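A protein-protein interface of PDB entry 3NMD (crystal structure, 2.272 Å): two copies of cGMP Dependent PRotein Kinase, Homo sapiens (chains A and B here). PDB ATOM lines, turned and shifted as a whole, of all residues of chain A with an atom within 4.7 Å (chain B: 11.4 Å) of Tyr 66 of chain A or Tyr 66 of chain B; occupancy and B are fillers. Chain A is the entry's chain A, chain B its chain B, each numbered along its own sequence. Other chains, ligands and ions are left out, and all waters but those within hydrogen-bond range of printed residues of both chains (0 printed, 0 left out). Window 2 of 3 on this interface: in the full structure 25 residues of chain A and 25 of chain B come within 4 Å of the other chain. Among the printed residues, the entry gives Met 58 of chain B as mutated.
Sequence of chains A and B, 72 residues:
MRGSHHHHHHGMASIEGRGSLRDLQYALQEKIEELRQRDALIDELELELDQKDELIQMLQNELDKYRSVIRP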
ATOM      1  N   GLU A  62      12.510 -19.146 -13.893  1.00  0.00           N
ATOM      2  CA  GLU A  62      13.770 -18.664 -14.434  1.00  0.00           C
ATOM      3  C   GLU A  62      13.590 -17.314 -15.144  1.00  0.00           C
ATOM      4  O   GLU A  62      14.349 -16.381 -14.902  1.00  0.00           O
ATOM      5  CB  GLU A  62      14.372 -19.704 -15.377  1.00  0.00           C
ATOM      6  CG  GLU A  62      15.795 -19.399 -15.808  1.00  0.00           C
ATOM      7  CD  GLU A  62      16.765 -19.375 -14.645  1.00  0.00           C
ATOM      8  OE1 GLU A  62      16.568 -20.160 -13.688  1.00  0.00           O
ATOM      9  OE2 GLU A  62      17.725 -18.574 -14.691  1.00  0.00           O
ATOM     10  N   LEU A  63      12.575 -17.209 -15.998  1.00  0.00           N
ATOM     11  CA  LEU A  63      12.319 -15.968 -16.735  1.00  0.00           C
ATOM     12  C   LEU A  63      11.992 -14.821 -15.801  1.00  0.00           C
ATOM     13  O   LEU A  63      12.330 -13.669 -16.077  1.00  0.00           O
ATOM     14  CB  LEU A  63      11.177 -16.144 -17.745  1.00  0.00           C
ATOM     15  CG  LEU A  63      11.515 -16.813 -19.083  1.00  0.00           C
ATOM     16  CD1 LEU A  63      10.253 -17.134 -19.874  1.00  0.00           C
ATOM     17  CD2 LEU A  63      12.435 -15.925 -19.907  1.00  0.00           C
ATOM     18  N   ASP A  64      11.329 -15.148 -14.695  1.00  0.00           N
ATOM     19  CA  ASP A  64      10.916 -14.156 -13.707  1.00  0.00           C
ATOM     20  C   ASP A  64      12.084 -13.528 -12.957  1.00  0.00           C
ATOM     21  O   ASP A  64      11.990 -12.385 -12.531  1.00  0.00           O
ATOM     22  CB  ASP A  64       9.905 -14.744 -12.718  1.00  0.00           C
ATOM     23  CG  ASP A  64       8.486 -14.723 -13.259  1.00  0.00           C
ATOM     24  OD1 ASP A  64       7.646 -15.499 -12.758  1.00  0.00           O
ATOM     25  OD2 ASP A  64       8.210 -13.930 -14.185  1.00  0.00           O
ATOM     26  N   LYS A  65      13.172 -14.272 -12.784  1.00  0.00           N
ATOM     27  CA  LYS A  65      14.409 -13.686 -12.269  1.00  0.00           C
ATOM     28  C   LYS A  65      14.736 -12.398 -13.030  1.00  0.00           C
ATOM     29  O   LYS A  65      15.200 -11.426 -12.446  1.00  0.00           O
ATOM     30  CB  LYS A  65      15.594 -14.646 -12.432  1.00  0.00           C
ATOM     31  CG  LYS A  65      15.669 -15.797 -11.444  1.00  0.00           C
ATOM     32  CD  LYS A  65      16.958 -16.592 -11.663  1.00  0.00           C
ATOM     33  CE  LYS A  65      17.158 -17.690 -10.618  1.00  0.00           C
ATOM     34  NZ  LYS A  65      16.240 -18.854 -10.802  1.00  0.00           N
ATOM     35  N   TYR A  66      14.498 -12.398 -14.341  1.00  0.00           N
ATOM     36  CA  TYR A  66      14.920 -11.274 -15.174  1.00  0.00           C
ATOM     37  C   TYR A  66      13.884 -10.152 -15.304  1.00  0.00           C
ATOM     38  O   TYR A  66      14.194  -9.067 -15.801  1.00  0.00           O
ATOM     39  CB  TYR A  66      15.365 -11.775 -16.546  1.00  0.00           C
ATOM     40  CG  TYR A  66      16.463 -12.812 -16.454  1.00  0.00           C
ATOM     41  CD1 TYR A  66      17.761 -12.444 -16.110  1.00  0.00           C
ATOM     42  CD2 TYR A  66      16.201 -14.159 -16.686  1.00  0.00           C
ATOM     43  CE1 TYR A  66      18.772 -13.381 -16.011  1.00  0.00           C
ATOM     44  CE2 TYR A  66      17.205 -15.113 -16.581  1.00  0.00           C
ATOM     45  CZ  TYR A  66      18.489 -14.715 -16.244  1.00  0.00           C
ATOM     46  OH  TYR A  66      19.499 -15.645 -16.140  1.00  0.00           O
ATOM     47  N   ARG A  67      12.666 -10.418 -14.843  1.00  0.00           N
ATOM     48  CA  ARG A  67      11.563  -9.472 -14.958  1.00  0.00           C
ATOM     49  C   ARG A  67      10.844  -9.257 -13.625  1.00  0.00           C
ATOM     50  O   ARG A  67       9.703  -8.802 -13.606  1.00  0.00           O
ATOM     51  CB  ARG A  67      10.536  -9.983 -15.971  1.00  0.00           C
ATOM     52  CG  ARG A  67      11.079 -10.329 -17.352  1.00  0.00           C
ATOM     53  CD  ARG A  67      10.020 -11.095 -18.143  1.00  0.00           C
ATOM     54  NE  ARG A  67      10.470 -11.469 -19.481  1.00  0.00           N
ATOM     55  CZ  ARG A  67       9.693 -12.028 -20.406  1.00  0.00           C
ATOM     56  NH1 ARG A  67       8.418 -12.284 -20.144  1.00  0.00           N
ATOM     57  NH2 ARG A  67      10.189 -12.332 -21.597  1.00  0.00           N
ATOM     58  N   SER A  68      11.500  -9.596 -12.519  1.00  0.00           N
ATOM     59  CA  SER A  68      10.874  -9.523 -11.197  1.00  0.00           C
ATOM     60  C   SER A  68      10.150  -8.204 -10.958  1.00  0.00           C
ATOM     61  O   SER A  68       8.963  -8.177 -10.624  1.00  0.00           O
ATOM     62  CB  SER A  68      11.920  -9.704 -10.093  1.00  0.00           C
ATOM     63  OG  SER A  68      12.529 -10.974 -10.160  1.00  0.00           O
ATOM     64  N   MET B  58       8.315 -22.586 -26.677  1.00  0.00           N
ATOM     65  CA  MET B  58       8.098 -21.144 -26.683  1.00  0.00           C
ATOM     66  C   MET B  58       8.839 -20.472 -25.520  1.00  0.00           C
ATOM     67  O   MET B  58       9.459 -19.419 -25.681  1.00  0.00           O
ATOM     68  CB  MET B  58       6.599 -20.848 -26.603  1.00  0.00           C
ATOM     69  CG  MET B  58       6.250 -19.374 -26.504  1.00  0.00           C
ATOM     70  SD  MET B  58       4.377 -19.037 -26.022  1.00  0.00           S
ATOM     71  CE  MET B  58       4.270 -20.112 -24.393  1.00  0.00           C
ATOM     72  N   LEU B  59       8.775 -21.094 -24.353  1.00  0.00           N
ATOM     73  CA  LEU B  59       9.417 -20.562 -23.159  1.00  0.00           C
ATOM     74  C   LEU B  59      10.951 -20.648 -23.241  1.00  0.00           C
ATOM     75  O   LEU B  59      11.650 -19.746 -22.776  1.00  0.00           O
ATOM     76  CB  LEU B  59       8.873 -21.266 -21.909  1.00  0.00           C
ATOM     77  CG  LEU B  59       7.469 -20.875 -21.411  1.00  0.00           C
ATOM     78  CD1 LEU B  59       7.013 -21.780 -20.269  1.00  0.00           C
ATOM     79  CD2 LEU B  59       7.422 -19.428 -20.965  1.00  0.00           C
ATOM     80  N   GLN B  60      11.471 -21.713 -23.851  1.00  0.00           N
ATOM     81  CA  GLN B  60      12.918 -21.848 -24.046  1.00  0.00           C
ATOM     82  C   GLN B  60      13.446 -20.794 -25.007  1.00  0.00           C
ATOM     83  O   GLN B  60      14.489 -20.183 -24.763  1.00  0.00           O
ATOM     84  CB  GLN B  60      13.293 -23.253 -24.537  1.00  0.00           C
ATOM     85  CG  GLN B  60      13.010 -24.337 -23.498  1.00  0.00           C
ATOM     86  CD  GLN B  60      13.219 -25.742 -24.028  1.00  0.00           C
ATOM     87  OE1 GLN B  60      13.574 -26.652 -23.278  1.00  0.00           O
ATOM     88  NE2 GLN B  60      12.999 -25.928 -25.327  1.00  0.00           N
ATOM     89  N   ASN B  61      12.716 -20.569 -26.092  1.00  0.00           N
ATOM     90  CA  ASN B  61      13.102 -19.521 -27.028  1.00  0.00           C
ATOM     91  C   ASN B  61      13.155 -18.160 -26.334  1.00  0.00           C
ATOM     92  O   ASN B  61      14.064 -17.357 -26.558  1.00  0.00           O
ATOM     93  CB  ASN B  61      12.149 -19.491 -28.223  1.00  0.00           C
ATOM     94  CG  ASN B  61      12.320 -20.697 -29.122  1.00  0.00           C
ATOM     95  OD1 ASN B  61      11.425 -21.049 -29.890  1.00  0.00           O
ATOM     96  ND2 ASN B  61      13.477 -21.341 -29.027  1.00  0.00           N
ATOM     97  N   GLU B  62      12.175 -17.919 -25.481  1.00  0.00           N
ATOM     98  CA  GLU B  62      12.138 -16.702 -24.680  1.00  0.00           C
ATOM     99  C   GLU B  62      13.358 -16.600 -23.748  1.00  0.00           C
ATOM    100  O   GLU B  62      14.007 -15.554 -23.675  1.00  0.00           O
ATOM    101  CB  GLU B  62      10.835 -16.657 -23.866  1.00  0.00           C
ATOM    102  CG  GLU B  62      10.441 -15.261 -23.419  1.00  0.00           C
ATOM    103  CD  GLU B  62      10.167 -14.342 -24.590  1.00  0.00           C
ATOM    104  OE1 GLU B  62      10.003 -14.853 -25.716  1.00  0.00           O
ATOM    105  OE2 GLU B  62      10.117 -13.112 -24.388  1.00  0.00           O
ATOM    106  N   LEU B  63      13.663 -17.688 -23.044  1.00  0.00           N
ATOM    107  CA  LEU B  63      14.788 -17.710 -22.104  1.00  0.00           C
ATOM    108  C   LEU B  63      16.110 -17.467 -22.831  1.00  0.00           C
ATOM    109  O   LEU B  63      17.030 -16.871 -22.283  1.00  0.00           O
ATOM    110  CB  LEU B  63      14.851 -19.056 -21.367  1.00  0.00           C
ATOM    111  CG  LEU B  63      15.119 -19.102 -19.856  1.00  0.00           C
ATOM    112  CD1 LEU B  63      15.940 -20.348 -19.513  1.00  0.00           C
ATOM    113  CD2 LEU B  63      15.800 -17.831 -19.309  1.00  0.00           C
ATOM    114  N   ASP B  64      16.198 -17.946 -24.069  1.00  0.00           N
ATOM    115  CA  ASP B  64      17.390 -17.749 -24.898  1.00  0.00           C
ATOM    116  C   ASP B  64      17.694 -16.272 -25.192  1.00  0.00           C
ATOM    117  O   ASP B  64      18.823 -15.928 -25.519  1.00  0.00           O
ATOM    118  CB  ASP B  64      17.272 -18.530 -26.213  1.00  0.00           C
ATOM    119  CG  ASP B  64      17.328 -20.036 -26.009  1.00  0.00           C
ATOM    120  OD1 ASP B  64      17.788 -20.481 -24.934  1.00  0.00           O
ATOM    121  OD2 ASP B  64      16.918 -20.778 -26.929  1.00  0.00           O
ATOM    122  N   LYS B  65      16.684 -15.409 -25.098  1.00  0.00           N
ATOM    123  CA  LYS B  65      16.905 -13.970 -25.240  1.00  0.00           C
ATOM    124  C   LYS B  65      17.681 -13.444 -24.047  1.00  0.00           C
ATOM    125  O   LYS B  65      18.440 -12.494 -24.170  1.00  0.00           O
ATOM    126  CB  LYS B  65      15.580 -13.207 -25.347  1.00  0.00           C
ATOM    127  CG  LYS B  65      14.747 -13.543 -26.574  1.00  0.00           C
ATOM    128  CD  LYS B  65      13.397 -12.844 -26.514  1.00  0.00           C
ATOM    129  CE  LYS B  65      12.524 -13.192 -27.715  1.00  0.00           C
ATOM    130  N   TYR B  66      17.481 -14.067 -22.888  1.00  0.00           N
ATOM    131  CA  TYR B  66      18.117 -13.612 -21.652  1.00  0.00           C
ATOM    132  C   TYR B  66      19.436 -14.326 -21.377  1.00  0.00           C
ATOM    133  O   TYR B  66      20.393 -13.714 -20.917  1.00  0.00           O
ATOM    134  CB  TYR B  66      17.159 -13.806 -20.462  1.00  0.00           C
ATOM    135  CG  TYR B  66      15.909 -12.960 -20.580  1.00  0.00           C
ATOM    136  CD1 TYR B  66      15.852 -11.696 -20.013  1.00  0.00           C
ATOM    137  CD2 TYR B  66      14.800 -13.413 -21.285  1.00  0.00           C
ATOM    138  CE1 TYR B  66      14.725 -10.906 -20.127  1.00  0.00           C
ATOM    139  CE2 TYR B  66      13.661 -12.621 -21.413  1.00  0.00           C
ATOM    140  CZ  TYR B  66      13.632 -11.372 -20.825  1.00  0.00           C
ATOM    141  OH  TYR B  66      12.521 -10.569 -20.943  1.00  0.00           O
ATOM    142  N   ARG B  67      19.468 -15.615 -21.690  1.00  0.00           N
ATOM    143  CA  ARG B  67      20.480 -16.542 -21.178  1.00  0.00           C
ATOM    144  C   ARG B  67      21.119 -16.083 -19.874  1.00  0.00           C
ATOM    145  O   ARG B  67      20.660 -16.444 -18.790  1.00  0.00           O
ATOM    146  CB  ARG B  67      21.546 -16.834 -22.220  1.00  0.00           C
ATOM    147  CG  ARG B  67      21.077 -17.757 -23.295  1.00  0.00           C
ATOM    148  CD  ARG B  67      22.238 -18.624 -23.789  1.00  0.00           C
ATOM    149  NE  ARG B  67      22.385 -19.826 -22.971  1.00  0.00           N
ATOM    150  CZ  ARG B  67      21.700 -20.949 -23.170  1.00  0.00           C
ATOM    151  NH1 ARG B  67      20.829 -21.026 -24.167  1.00  0.00           N
ATOM    152  NH2 ARG B  67      21.883 -21.995 -22.376  1.00  0.00           N
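Among the printed residues, pairs that only touch across the chains: Glu 62 of chain A with Leu 63 of chain B (3.8 Å), Leu 63 of chain A with Leu 59 of chain B (3.8 Å), Leu 63 of chain A with Leu 63 of chain B (3.7 Å), Leu 63 of chain A with Tyr 66 of chain B (3.7 Å) and Tyr 66 of chain A with Tyr 66 of chain B (3.5 Å).
Of the 7 printed residues of chain A, 4 touch a printed residue of chain B.
Printed residues of chain A that touch a printed residue of chain B: Glu 62, Leu 63, Tyr 66 and Arg 67.
Hydrophobic or aromatic side chains of chain A within 4 Å of the printed part of chain B: Leu 63 and Tyr 66.
Printed residues of chain B that touch a printed residue of chain A: Leu 59, Glu 62, Leu 63, Tyr 66 and Arg 67.
Hydrophobic or aromatic side chains of chain B within 4 Å of the printed part of chain A: Leu 59, Leu 63 and Tyr 66.
Among the printed residues, 8 pairs touch across the chains.
Among the printed residues, Asp or Glu carboxylates within 4 Å of a Lys or Arg side-chain nitrogen of the other chain: Arg 67 of chain A with Glu 62 of chain B (2.9 Å).
Tyr 66 of chain A touches just these residues of chain B: Tyr 66 and Arg 67.
Tyr 66 of chain B touches three residues of chain A.
Of the printed residues of chain A, Arg 67 of chain B touches Tyr 66 (3.0 Å).
Of the printed residues of chain B, Leu 63 of chain A touches Leu 59, Leu 63 and Tyr 66.
The nearest printed residue of chain A that does not touch Tyr 66 of chain B is Glu 62 of chain A (6.7 Å).
The nearest printed residue of chain A that does not touch Leu 59 of chain B is Arg 67 of chain A (7.3 Å).
The guanidinium group (NH1) of Arg 67 of chain B is in salt-bridge range of the side-chain carboxylate (OD1) of Asp 64 of chain B (3.2 Å).
The side-chain amino group (NZ) of Lys 65 of chain A lies within salt-bridge range of the side-chain carboxylate (OE1) of Glu 62 of chain A (3.2 Å).
OH of Tyr 66 of chain A lies within hydrogen-bond range of O of Arg 67 of chain B (3.0 Å).
NH2 of Arg 67 of chain A lies within salt-bridge range of OE2 of Glu 62 of chain B (2.9 Å).
NE of Arg 67 of chain A is in hydrogen-bond range of OH of Tyr 66 of chain B (2.7 Å).
Glu 62 of chain A touches Leu 63 of chain B, but with the chains exchanged Leu 63 of chain A does not touch Glu 62 of chain B (4.01 Å).
Leu 63 of chain A touches its own counterpart, Leu 63 of chain B.
Tyr 66 of chain A touches Arg 67 of chain B, and with the chains exchanged Arg 67 of chain A touches Tyr 66 of chain B.
Arg 67 of chain A touches Glu 62 of chain B, but with the chains exchanged Glu 62 of chain A does not touch Arg 67 of chain B (5.5 Å).
Positions printed for both chains: 62, 63, 64, 65, 66 and 67.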
